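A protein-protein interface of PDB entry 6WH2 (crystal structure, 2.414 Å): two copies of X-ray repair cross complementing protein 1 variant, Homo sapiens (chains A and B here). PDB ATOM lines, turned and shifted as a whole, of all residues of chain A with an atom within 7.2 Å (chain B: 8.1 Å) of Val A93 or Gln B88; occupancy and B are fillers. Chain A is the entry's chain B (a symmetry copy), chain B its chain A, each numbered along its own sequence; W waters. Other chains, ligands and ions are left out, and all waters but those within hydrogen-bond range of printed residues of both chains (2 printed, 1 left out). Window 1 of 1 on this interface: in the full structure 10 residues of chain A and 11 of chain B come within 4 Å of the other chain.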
ATOM      1  N   GLN A  51      15.246 -38.667  15.218  1.00  0.00           N
ATOM      2  CA  GLN A  51      15.882 -38.820  13.921  1.00  0.00           C
ATOM      3  C   GLN A  51      17.205 -38.058  13.879  1.00  0.00           C
ATOM      4  O   GLN A  51      17.689 -37.545  14.892  1.00  0.00           O
ATOM      5  CB  GLN A  51      14.940 -38.344  12.815  1.00  0.00           C
ATOM      6  CG  GLN A  51      13.626 -39.093  12.733  1.00  0.00           C
ATOM      7  CD  GLN A  51      12.980 -38.945  11.373  1.00  0.00           C
ATOM      8  OE1 GLN A  51      11.914 -38.344  11.238  1.00  0.00           O
ATOM      9  NE2 GLN A  51      13.631 -39.486  10.350  1.00  0.00           N
ATOM     10  N   GLU A  52      17.803 -37.981  12.693  1.00  0.00           N
ATOM     11  CA  GLU A  52      19.072 -37.286  12.560  1.00  0.00           C
ATOM     12  C   GLU A  52      18.880 -35.777  12.653  1.00  0.00           C
ATOM     13  O   GLU A  52      17.765 -35.252  12.560  1.00  0.00           O
ATOM     14  CB  GLU A  52      19.756 -37.620  11.231  1.00  0.00           C
ATOM     15  CG  GLU A  52      20.740 -38.769  11.247  1.00  0.00           C
ATOM     16  CD  GLU A  52      21.406 -38.975  12.579  1.00  0.00           C
ATOM     17  OE1 GLU A  52      21.369 -40.117  13.082  1.00  0.00           O
ATOM     18  OE2 GLU A  52      21.977 -38.025  13.145  1.00  0.00           O
ATOM     19  N   TRP A  53      20.003 -35.080  12.828  1.00  0.00           N
ATOM     20  CA  TRP A  53      20.007 -33.625  12.823  1.00  0.00           C
ATOM     21  C   TRP A  53      19.527 -33.111  11.476  1.00  0.00           C
ATOM     22  O   TRP A  53      19.995 -33.555  10.424  1.00  0.00           O
ATOM     23  CB  TRP A  53      21.414 -33.101  13.120  1.00  0.00           C
ATOM     24  CG  TRP A  53      21.469 -31.626  13.274  1.00  0.00           C
ATOM     25  CD1 TRP A  53      21.682 -30.711  12.288  1.00  0.00           C
ATOM     26  CD2 TRP A  53      21.305 -30.883  14.487  1.00  0.00           C
ATOM     27  NE1 TRP A  53      21.661 -29.443  12.811  1.00  0.00           N
ATOM     28  CE2 TRP A  53      21.432 -29.521  14.158  1.00  0.00           C
ATOM     29  CE3 TRP A  53      21.064 -31.238  15.818  1.00  0.00           C
ATOM     30  CZ2 TRP A  53      21.325 -28.510  15.112  1.00  0.00           C
ATOM     31  CZ3 TRP A  53      20.959 -30.231  16.766  1.00  0.00           C
ATOM     32  CH2 TRP A  53      21.089 -28.884  16.406  1.00  0.00           C
ATOM     33  N   LEU A  61      17.867 -21.980  14.679  1.00  0.00           N
ATOM     34  CA  LEU A  61      18.721 -21.453  15.739  1.00  0.00           C
ATOM     35  C   LEU A  61      19.112 -20.003  15.493  1.00  0.00           C
ATOM     36  O   LEU A  61      19.310 -19.248  16.451  1.00  0.00           O
ATOM     37  CB  LEU A  61      19.973 -22.317  15.885  1.00  0.00           C
ATOM     38  CG  LEU A  61      19.817 -23.635  16.639  1.00  0.00           C
ATOM     39  CD1 LEU A  61      20.886 -24.628  16.208  1.00  0.00           C
ATOM     40  CD2 LEU A  61      19.879 -23.393  18.138  1.00  0.00           C
ATOM     41  N   ASN A  64      16.421 -18.231  16.962  1.00  0.00           N
ATOM     42  CA  ASN A  64      16.115 -18.687  18.318  1.00  0.00           C
ATOM     43  C   ASN A  64      17.371 -19.318  18.905  1.00  0.00           C
ATOM     44  O   ASN A  64      17.535 -20.544  18.878  1.00  0.00           O
ATOM     45  CB  ASN A  64      14.945 -19.674  18.309  1.00  0.00           C
ATOM     46  CG  ASN A  64      14.347 -19.889  19.682  1.00  0.00           C
ATOM     47  OD1 ASN A  64      14.789 -19.301  20.665  1.00  0.00           O
ATOM     48  ND2 ASN A  64      13.328 -20.736  19.755  1.00  0.00           N
ATOM     49  N   PRO A  65      18.284 -18.504  19.442  1.00  0.00           N
ATOM     50  CA  PRO A  65      19.552 -19.063  19.945  1.00  0.00           C
ATOM     51  C   PRO A  65      19.394 -19.990  21.141  1.00  0.00           C
ATOM     52  O   PRO A  65      20.216 -20.897  21.312  1.00  0.00           O
ATOM     53  CB  PRO A  65      20.366 -17.812  20.308  1.00  0.00           C
ATOM     54  CG  PRO A  65      19.750 -16.705  19.515  1.00  0.00           C
ATOM     55  CD  PRO A  65      18.290 -17.031  19.442  1.00  0.00           C
ATOM     56  N   SER A  66      18.371 -19.797  21.975  1.00  0.00           N
ATOM     57  CA  SER A  66      18.214 -20.617  23.170  1.00  0.00           C
ATOM     58  C   SER A  66      17.592 -21.979  22.887  1.00  0.00           C
ATOM     59  O   SER A  66      17.335 -22.727  23.838  1.00  0.00           O
ATOM     60  CB  SER A  66      17.367 -19.883  24.215  1.00  0.00           C
ATOM     61  OG  SER A  66      16.142 -19.439  23.660  1.00  0.00           O
ATOM     62  N   LEU A  67      17.350 -22.316  21.622  1.00  0.00           N
ATOM     63  CA  LEU A  67      16.702 -23.576  21.285  1.00  0.00           C
ATOM     64  C   LEU A  67      17.521 -24.763  21.777  1.00  0.00           C
ATOM     65  O   LEU A  67      18.753 -24.763  21.709  1.00  0.00           O
ATOM     66  CB  LEU A  67      16.501 -23.676  19.772  1.00  0.00           C
ATOM     67  CG  LEU A  67      15.070 -23.584  19.237  1.00  0.00           C
ATOM     68  CD1 LEU A  67      15.074 -23.607  17.718  1.00  0.00           C
ATOM     69  CD2 LEU A  67      14.211 -24.710  19.791  1.00  0.00           C
ATOM     70  N   ALA A  68      16.824 -25.780  22.279  1.00  0.00           N
ATOM     71  CA  ALA A  68      17.436 -27.022  22.720  1.00  0.00           C
ATOM     72  C   ALA A  68      16.830 -28.184  21.947  1.00  0.00           C
ATOM     73  O   ALA A  68      15.621 -28.214  21.699  1.00  0.00           O
ATOM     74  CB  ALA A  68      17.246 -27.234  24.226  1.00  0.00           C
ATOM     75  N   PHE A  69      17.675 -29.140  21.566  1.00  0.00           N
ATOM     76  CA  PHE A  69      17.262 -30.299  20.782  1.00  0.00           C
ATOM     77  C   PHE A  69      17.526 -31.552  21.606  1.00  0.00           C
ATOM     78  O   PHE A  69      18.679 -31.848  21.938  1.00  0.00           O
ATOM     79  CB  PHE A  69      18.007 -30.347  19.446  1.00  0.00           C
ATOM     80  CG  PHE A  69      17.831 -29.105  18.613  1.00  0.00           C
ATOM     81  CD1 PHE A  69      18.672 -28.016  18.778  1.00  0.00           C
ATOM     82  CD2 PHE A  69      16.820 -29.026  17.668  1.00  0.00           C
ATOM     83  CE1 PHE A  69      18.510 -26.873  18.015  1.00  0.00           C
ATOM     84  CE2 PHE A  69      16.654 -27.887  16.903  1.00  0.00           C
ATOM     85  CZ  PHE A  69      17.500 -26.809  17.077  1.00  0.00           C
ATOM     86  N   HIS A  87      17.954 -31.326  30.261  1.00  0.00           N
ATOM     87  CA  HIS A  87      17.878 -31.743  28.866  1.00  0.00           C
ATOM     88  C   HIS A  87      19.248 -32.074  28.291  1.00  0.00           C
ATOM     89  O   HIS A  87      19.331 -32.835  27.321  1.00  0.00           O
ATOM     90  CB  HIS A  87      17.220 -30.647  28.026  1.00  0.00           C
ATOM     91  CG  HIS A  87      18.002 -29.372  27.984  1.00  0.00           C
ATOM     92  ND1 HIS A  87      18.954 -29.114  27.023  1.00  0.00           N
ATOM     93  CD2 HIS A  87      17.977 -28.284  28.791  1.00  0.00           C
ATOM     94  CE1 HIS A  87      19.480 -27.920  27.236  1.00  0.00           C
ATOM     95  NE2 HIS A  87      18.904 -27.396  28.303  1.00  0.00           N
ATOM     96  N   TYR A  90      20.318 -35.637  27.464  1.00  0.00           N
ATOM     97  CA  TYR A  90      19.688 -36.345  26.356  1.00  0.00           C
ATOM     98  C   TYR A  90      19.753 -35.520  25.072  1.00  0.00           C
ATOM     99  O   TYR A  90      18.917 -35.691  24.178  1.00  0.00           O
ATOM    100  CB  TYR A  90      18.231 -36.694  26.686  1.00  0.00           C
ATOM    101  CG  TYR A  90      18.035 -37.248  28.085  1.00  0.00           C
ATOM    102  CD1 TYR A  90      17.837 -36.399  29.168  1.00  0.00           C
ATOM    103  CD2 TYR A  90      18.051 -38.617  28.321  1.00  0.00           C
ATOM    104  CE1 TYR A  90      17.664 -36.898  30.446  1.00  0.00           C
ATOM    105  CE2 TYR A  90      17.875 -39.123  29.595  1.00  0.00           C
ATOM    106  CZ  TYR A  90      17.683 -38.260  30.653  1.00  0.00           C
ATOM    107  OH  TYR A  90      17.511 -38.759  31.923  1.00  0.00           O
ATOM    108  N   GLY A  91      20.746 -34.639  24.961  1.00  0.00           N
ATOM    109  CA  GLY A  91      20.778 -33.692  23.865  1.00  0.00           C
ATOM    110  C   GLY A  91      21.147 -34.321  22.534  1.00  0.00           C
ATOM    111  O   GLY A  91      21.718 -35.410  22.452  1.00  0.00           O
ATOM    112  N   VAL A  92      20.811 -33.595  21.470  1.00  0.00           N
ATOM    113  CA  VAL A  92      21.031 -34.027  20.096  1.00  0.00           C
ATOM    114  C   VAL A  92      21.935 -33.016  19.406  1.00  0.00           C
ATOM    115  O   VAL A  92      21.769 -31.803  19.575  1.00  0.00           O
ATOM    116  CB  VAL A  92      19.695 -34.181  19.337  1.00  0.00           C
ATOM    117  CG1 VAL A  92      19.934 -34.696  17.930  1.00  0.00           C
ATOM    118  CG2 VAL A  92      18.762 -35.110  20.095  1.00  0.00           C
ATOM    119  N   VAL A  93      22.897 -33.518  18.634  1.00  0.00           N
ATOM    120  CA  VAL A  93      23.865 -32.678  17.931  1.00  0.00           C
ATOM    121  C   VAL A  93      24.064 -33.223  16.525  1.00  0.00           C
ATOM    122  O   VAL A  93      23.736 -34.383  16.240  1.00  0.00           O
ATOM    123  CB  VAL A  93      25.218 -32.617  18.671  1.00  0.00           C
ATOM    124  CG1 VAL A  93      25.073 -31.886  19.998  1.00  0.00           C
ATOM    125  CG2 VAL A  93      25.771 -34.017  18.880  1.00  0.00           C
ATOM    126  N   PRO A  94      24.584 -32.396  15.613  1.00  0.00           N
ATOM    127  CA  PRO A  94      24.903 -32.896  14.271  1.00  0.00           C
ATOM    128  C   PRO A  94      25.921 -34.025  14.323  1.00  0.00           C
ATOM    129  O   PRO A  94      26.731 -34.123  15.248  1.00  0.00           O
ATOM    130  CB  PRO A  94      25.467 -31.663  13.558  1.00  0.00           C
ATOM    131  CG  PRO A  94      24.849 -30.511  14.268  1.00  0.00           C
ATOM    132  CD  PRO A  94      24.730 -30.931  15.703  1.00  0.00           C
ATOM    133  N   GLN A  95      25.873 -34.886  13.309  1.00  0.00           N
ATOM    134  CA  GLN A  95      26.665 -36.107  13.284  1.00  0.00           C
ATOM    135  C   GLN A  95      27.369 -36.240  11.938  1.00  0.00           C
ATOM    136  O   GLN A  95      27.164 -35.440  11.019  1.00  0.00           O
ATOM    137  CB  GLN A  95      25.784 -37.333  13.562  1.00  0.00           C
ATOM    138  CG  GLN A  95      26.468 -38.426  14.365  1.00  0.00           C
ATOM    139  CD  GLN A  95      26.841 -37.979  15.762  1.00  0.00           C
ATOM    140  OE1 GLN A  95      26.250 -37.049  16.312  1.00  0.00           O
ATOM    141  NE2 GLN A  95      27.832 -38.640  16.347  1.00  0.00           N
ATOM    142  N   ALA A  96      28.211 -37.270  11.841  1.00  0.00           N
ATOM    143  CA  ALA A  96      28.931 -37.628  10.618  1.00  0.00           C
ATOM    144  C   ALA A  96      29.606 -36.431   9.955  1.00  0.00           C
ATOM    145  O   ALA A  96      30.273 -35.630  10.611  1.00  0.00           O
ATOM    146  CB  ALA A  96      27.988 -38.309   9.635  1.00  0.00           C
ATOM    147  OXT ALA A  96      29.496 -36.241   8.744  1.00  0.00           O
ATOM    148  N   PHE B  46      30.165 -22.208  29.863  1.00  0.00           N
ATOM    149  CA  PHE B  46      30.511 -23.086  28.751  1.00  0.00           C
ATOM    150  C   PHE B  46      31.753 -23.883  29.113  1.00  0.00           C
ATOM    151  O   PHE B  46      32.821 -23.303  29.334  1.00  0.00           O
ATOM    152  CB  PHE B  46      30.747 -22.286  27.466  1.00  0.00           C
ATOM    153  CG  PHE B  46      29.564 -21.474  27.029  1.00  0.00           C
ATOM    154  CD1 PHE B  46      28.592 -22.026  26.211  1.00  0.00           C
ATOM    155  CD2 PHE B  46      29.422 -20.157  27.436  1.00  0.00           C
ATOM    156  CE1 PHE B  46      27.501 -21.281  25.807  1.00  0.00           C
ATOM    157  CE2 PHE B  46      28.333 -19.407  27.035  1.00  0.00           C
ATOM    158  CZ  PHE B  46      27.371 -19.970  26.220  1.00  0.00           C
ATOM    159  N   ALA B  68      26.468 -25.462  29.565  1.00  0.00           N
ATOM    160  CA  ALA B  68      26.595 -26.035  28.233  1.00  0.00           C
ATOM    161  C   ALA B  68      27.970 -26.670  28.072  1.00  0.00           C
ATOM    162  O   ALA B  68      28.973 -26.130  28.550  1.00  0.00           O
ATOM    163  CB  ALA B  68      26.381 -24.973  27.149  1.00  0.00           C
ATOM    164  N   PHE B  69      28.011 -27.817  27.396  1.00  0.00           N
ATOM    165  CA  PHE B  69      29.244 -28.557  27.149  1.00  0.00           C
ATOM    166  C   PHE B  69      29.496 -28.581  25.648  1.00  0.00           C
ATOM    167  O   PHE B  69      28.704 -29.155  24.894  1.00  0.00           O
ATOM    168  CB  PHE B  69      29.154 -29.980  27.706  1.00  0.00           C
ATOM    169  CG  PHE B  69      28.787 -30.042  29.166  1.00  0.00           C
ATOM    170  CD1 PHE B  69      27.460 -29.993  29.566  1.00  0.00           C
ATOM    171  CD2 PHE B  69      29.769 -30.156  30.135  1.00  0.00           C
ATOM    172  CE1 PHE B  69      27.123 -30.052  30.905  1.00  0.00           C
ATOM    173  CE2 PHE B  69      29.437 -30.215  31.477  1.00  0.00           C
ATOM    174  CZ  PHE B  69      28.112 -30.165  31.861  1.00  0.00           C
ATOM    175  N   VAL B  70      30.592 -27.956  25.215  1.00  0.00           N
ATOM    176  CA  VAL B  70      30.840 -27.725  23.798  1.00  0.00           C
ATOM    177  C   VAL B  70      32.239 -28.204  23.425  1.00  0.00           C
ATOM    178  O   VAL B  70      33.146 -28.259  24.262  1.00  0.00           O
ATOM    179  CB  VAL B  70      30.664 -26.235  23.423  1.00  0.00           C
ATOM    180  CG1 VAL B  70      30.415 -26.092  21.936  1.00  0.00           C
ATOM    181  CG2 VAL B  70      29.525 -25.605  24.215  1.00  0.00           C
ATOM    182  N   ARG B  71      32.404 -28.545  22.147  1.00  0.00           N
ATOM    183  CA  ARG B  71      33.672 -28.985  21.588  1.00  0.00           C
ATOM    184  C   ARG B  71      34.545 -27.788  21.219  1.00  0.00           C
ATOM    185  O   ARG B  71      34.047 -26.675  21.032  1.00  0.00           O
ATOM    186  CB  ARG B  71      33.424 -29.844  20.350  1.00  0.00           C
ATOM    187  CG  ARG B  71      32.846 -31.218  20.638  1.00  0.00           C
ATOM    188  CD  ARG B  71      33.797 -32.056  21.470  1.00  0.00           C
ATOM    189  NE  ARG B  71      33.362 -33.446  21.548  1.00  0.00           N
ATOM    190  CZ  ARG B  71      33.692 -34.276  22.532  1.00  0.00           C
ATOM    191  NH1 ARG B  71      34.460 -33.853  23.526  1.00  0.00           N
ATOM    192  NH2 ARG B  71      33.254 -35.527  22.524  1.00  0.00           N
ATOM    193  N   TRP B  74      33.758 -25.430  18.068  1.00  0.00           N
ATOM    194  CA  TRP B  74      32.884 -24.264  18.153  1.00  0.00           C
ATOM    195  C   TRP B  74      33.689 -22.974  18.171  1.00  0.00           C
ATOM    196  O   TRP B  74      33.335 -22.000  17.497  1.00  0.00           O
ATOM    197  CB  TRP B  74      32.010 -24.365  19.403  1.00  0.00           C
ATOM    198  CG  TRP B  74      31.149 -23.165  19.663  1.00  0.00           C
ATOM    199  CD1 TRP B  74      30.395 -22.483  18.753  1.00  0.00           C
ATOM    200  CD2 TRP B  74      30.949 -22.510  20.922  1.00  0.00           C
ATOM    201  NE1 TRP B  74      29.739 -21.443  19.368  1.00  0.00           N
ATOM    202  CE2 TRP B  74      30.062 -21.438  20.698  1.00  0.00           C
ATOM    203  CE3 TRP B  74      31.435 -22.724  22.215  1.00  0.00           C
ATOM    204  CZ2 TRP B  74      29.650 -20.584  21.720  1.00  0.00           C
ATOM    205  CZ3 TRP B  74      31.025 -21.876  23.229  1.00  0.00           C
ATOM    206  CH2 TRP B  74      30.142 -20.819  22.975  1.00  0.00           C
ATOM    207  N   LEU B  85      28.461 -18.401  16.581  1.00  0.00           N
ATOM    208  CA  LEU B  85      27.657 -19.493  16.061  1.00  0.00           C
ATOM    209  C   LEU B  85      27.010 -20.261  17.203  1.00  0.00           C
ATOM    210  O   LEU B  85      27.502 -20.243  18.335  1.00  0.00           O
ATOM    211  CB  LEU B  85      28.524 -20.436  15.218  1.00  0.00           C
ATOM    212  CG  LEU B  85      29.363 -19.775  14.123  1.00  0.00           C
ATOM    213  CD1 LEU B  85      30.265 -20.797  13.453  1.00  0.00           C
ATOM    214  CD2 LEU B  85      28.471 -19.091  13.097  1.00  0.00           C
ATOM    215  N   PRO B  86      25.889 -20.936  16.948  1.00  0.00           N
ATOM    216  CA  PRO B  86      25.217 -21.675  18.025  1.00  0.00           C
ATOM    217  C   PRO B  86      26.098 -22.786  18.577  1.00  0.00           C
ATOM    218  O   PRO B  86      26.657 -23.591  17.830  1.00  0.00           O
ATOM    219  CB  PRO B  86      23.962 -22.233  17.342  1.00  0.00           C
ATOM    220  CG  PRO B  86      23.739 -21.340  16.169  1.00  0.00           C
ATOM    221  CD  PRO B  86      25.108 -20.952  15.700  1.00  0.00           C
ATOM    222  N   HIS B  87      26.218 -22.818  19.907  1.00  0.00           N
ATOM    223  CA  HIS B  87      26.981 -23.877  20.560  1.00  0.00           C
ATOM    224  C   HIS B  87      26.327 -25.237  20.367  1.00  0.00           C
ATOM    225  O   HIS B  87      27.004 -26.269  20.445  1.00  0.00           O
ATOM    226  CB  HIS B  87      27.128 -23.571  22.050  1.00  0.00           C
ATOM    227  CG  HIS B  87      25.831 -23.597  22.798  1.00  0.00           C
ATOM    228  ND1 HIS B  87      25.080 -22.464  23.026  1.00  0.00           N
ATOM    229  CD2 HIS B  87      25.146 -24.620  23.361  1.00  0.00           C
ATOM    230  CE1 HIS B  87      23.992 -22.787  23.701  1.00  0.00           C
ATOM    231  NE2 HIS B  87      24.008 -24.089  23.918  1.00  0.00           N
ATOM    232  N   GLN B  88      25.014 -25.258  20.116  1.00  0.00           N
ATOM    233  CA  GLN B  88      24.302 -26.522  19.957  1.00  0.00           C
ATOM    234  C   GLN B  88      24.828 -27.322  18.772  1.00  0.00           C
ATOM    235  O   GLN B  88      24.725 -28.554  18.761  1.00  0.00           O
ATOM    236  CB  GLN B  88      22.804 -26.258  19.795  1.00  0.00           C
ATOM    237  CG  GLN B  88      22.148 -25.612  21.009  1.00  0.00           C
ATOM    238  CD  GLN B  88      22.098 -24.099  20.913  1.00  0.00           C
ATOM    239  OE1 GLN B  88      22.943 -23.478  20.269  1.00  0.00           O
ATOM    240  NE2 GLN B  88      21.102 -23.499  21.555  1.00  0.00           N
ATOM    241  N   LEU B  89      25.397 -26.646  17.771  1.00  0.00           N
ATOM    242  CA  LEU B  89      25.950 -27.331  16.609  1.00  0.00           C
ATOM    243  C   LEU B  89      27.240 -28.079  16.920  1.00  0.00           C
ATOM    244  O   LEU B  89      27.704 -28.853  16.076  1.00  0.00           O
ATOM    245  CB  LEU B  89      26.197 -26.328  15.482  1.00  0.00           C
ATOM    246  CG  LEU B  89      24.972 -25.572  14.965  1.00  0.00           C
ATOM    247  CD1 LEU B  89      25.396 -24.440  14.047  1.00  0.00           C
ATOM    248  CD2 LEU B  89      24.028 -26.517  14.246  1.00  0.00           C
ATOM    249  N   TYR B  90      27.829 -27.868  18.100  1.00  0.00           N
ATOM    250  CA  TYR B  90      29.092 -28.499  18.470  1.00  0.00           C
ATOM    251  C   TYR B  90      29.043 -29.074  19.881  1.00  0.00           C
ATOM    252  O   TYR B  90      30.089 -29.228  20.518  1.00  0.00           O
ATOM    253  CB  TYR B  90      30.251 -27.503  18.349  1.00  0.00           C
ATOM    254  CG  TYR B  90      30.225 -26.671  17.085  1.00  0.00           C
ATOM    255  CD1 TYR B  90      29.507 -25.482  17.025  1.00  0.00           C
ATOM    256  CD2 TYR B  90      30.921 -27.073  15.953  1.00  0.00           C
ATOM    257  CE1 TYR B  90      29.479 -24.721  15.873  1.00  0.00           C
ATOM    258  CE2 TYR B  90      30.900 -26.317  14.796  1.00  0.00           C
ATOM    259  CZ  TYR B  90      30.177 -25.143  14.761  1.00  0.00           C
ATOM    260  OH  TYR B  90      30.152 -24.387  13.612  1.00  0.00           O
ATOM    261  N   GLY B  91      27.852 -29.403  20.376  1.00  0.00           N
ATOM    262  CA  GLY B  91      27.712 -29.790  21.763  1.00  0.00           C
ATOM    263  C   GLY B  91      28.217 -31.191  22.047  1.00  0.00           C
ATOM    264  O   GLY B  91      28.363 -32.035  21.161  1.00  0.00           O
ATOM    265  N   VAL B  92      28.493 -31.430  23.326  1.00  0.00           N
ATOM    266  CA  VAL B  92      28.910 -32.732  23.832  1.00  0.00           C
ATOM    267  C   VAL B  92      27.742 -33.331  24.600  1.00  0.00           C
ATOM    268  O   VAL B  92      27.192 -32.692  25.504  1.00  0.00           O
ATOM    269  CB  VAL B  92      30.157 -32.617  24.726  1.00  0.00           C
ATOM    270  CG1 VAL B  92      30.689 -33.996  25.081  1.00  0.00           C
ATOM    271  CG2 VAL B  92      31.226 -31.783  24.039  1.00  0.00           C
ATOM    272  N   VAL B  93      27.359 -34.553  24.238  1.00  0.00           N
ATOM    273  CA  VAL B  93      26.184 -35.196  24.820  1.00  0.00           C
ATOM    274  C   VAL B  93      26.553 -36.621  25.209  1.00  0.00           C
ATOM    275  O   VAL B  93      27.527 -37.190  24.690  1.00  0.00           O
ATOM    276  CB  VAL B  93      24.980 -35.172  23.848  1.00  0.00           C
ATOM    277  CG1 VAL B  93      24.506 -33.742  23.627  1.00  0.00           C
ATOM    278  CG2 VAL B  93      25.350 -35.825  22.528  1.00  0.00           C
ATOM    279  N   PRO B  94      25.799 -37.227  26.135  1.00  0.00           N
ATOM    280  CA  PRO B  94      26.144 -38.584  26.596  1.00  0.00           C
ATOM    281  C   PRO B  94      26.022 -39.666  25.533  1.00  0.00           C
ATOM    282  O   PRO B  94      26.450 -40.797  25.799  1.00  0.00           O
ATOM    283  CB  PRO B  94      25.149 -38.832  27.739  1.00  0.00           C
ATOM    284  CG  PRO B  94      24.745 -37.477  28.194  1.00  0.00           C
ATOM    285  CD  PRO B  94      24.740 -36.623  26.964  1.00  0.00           C
ATOM    286  N   GLN B  95      25.465 -39.363  24.363  1.00  0.00           N
ATOM    287  CA  GLN B  95      25.171 -40.367  23.336  1.00  0.00           C
ATOM    288  C   GLN B  95      24.217 -41.429  23.874  1.00  0.00           C
ATOM    289  O   GLN B  95      24.576 -42.603  23.982  1.00  0.00           O
ATOM    290  CB  GLN B  95      26.452 -41.032  22.820  1.00  0.00           C
ATOM    291  CG  GLN B  95      27.407 -40.105  22.094  1.00  0.00           C
ATOM    292  CD  GLN B  95      28.630 -40.836  21.572  1.00  0.00           C
ATOM    293  OE1 GLN B  95      29.365 -41.465  22.334  1.00  0.00           O
ATOM    294  NE2 GLN B  95      28.852 -40.761  20.264  1.00  0.00           N
HETATM  295  O   HOH W   1      22.950 -20.474  20.530  1.00  0.00           O
HETATM  296  O   HOH W   2      22.492 -29.486  20.526  1.00  0.00           O
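Printed residues of chain B within 4 Å of Trp A53: Leu B89. Of the printed residues of chain B, Leu A61 touches Pro B86 (3.9 Å) and Gln B88 (3.6 Å). Val A93 touches two residues of chain B. Of chain B, only Gln B88 (3.9 Å) and Leu B89 (3.6 Å) come within 4 Å of Pro A94. Of chain A, only Leu A61, Pro A65, Leu A67, Val A93 and Pro A94 come within 4 Å of Gln B88. The nearest printed residue of chain B that does not touch Leu A67 is His B87 (5.7 Å).
O of Leu A67 is in hydrogen-bond range of NE2 of Gln B88 (2.7 Å). O of Pro A65 is in hydrogen-bond range of NE2 of Gln B88 (2.8 Å).
Of the 18 printed residues of chain A, 7 touch a printed residue of chain B. Hydrophobic or aromatic side chains of chain A that line the printed part of chain B: Trp A53, Leu A61, Val A93 and Pro A94. Of the 17 printed residues of chain B, 5 touch a printed residue of chain A. Printed residues of chain B that touch a printed residue of chain A: Pro B86, Gln B88, Leu B89, Gly B91 and Val B93. Among the printed residues, no Asp or Glu carboxylate lies within 4 Å of a Lys or Arg side-chain nitrogen of the other chain.
Water W2 lies within hydrogen-bond range of the backbone carbonyl oxygen of Val A92 and the backbone carbonyl oxygen of Gln B88. Water W1 bridges the backbone carbonyl oxygen of Pro A65 (2.9 Å) and the side-chain amide oxygen of Gln B88 (3.0 Å).
Among the printed residues, pairs that only touch across the chains: Gly A91 with Val B93 (3.5 Å), Trp A53 with Leu B89 (3.5 Å), Val A93 with Gly B91 (3.5 Å), Val A93 with Gln B88 (3.6 Å), Leu A61 with Gln B88 (3.6 Å), Pro A94 with Leu B89 (3.6 Å), Pro A94 with Gln B88 (3.9 Å) and Leu A61 with Pro B86 (3.9 Å).
Gly A91 touches Val B93, and with the chains exchanged Val A93 touches Gly B91.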
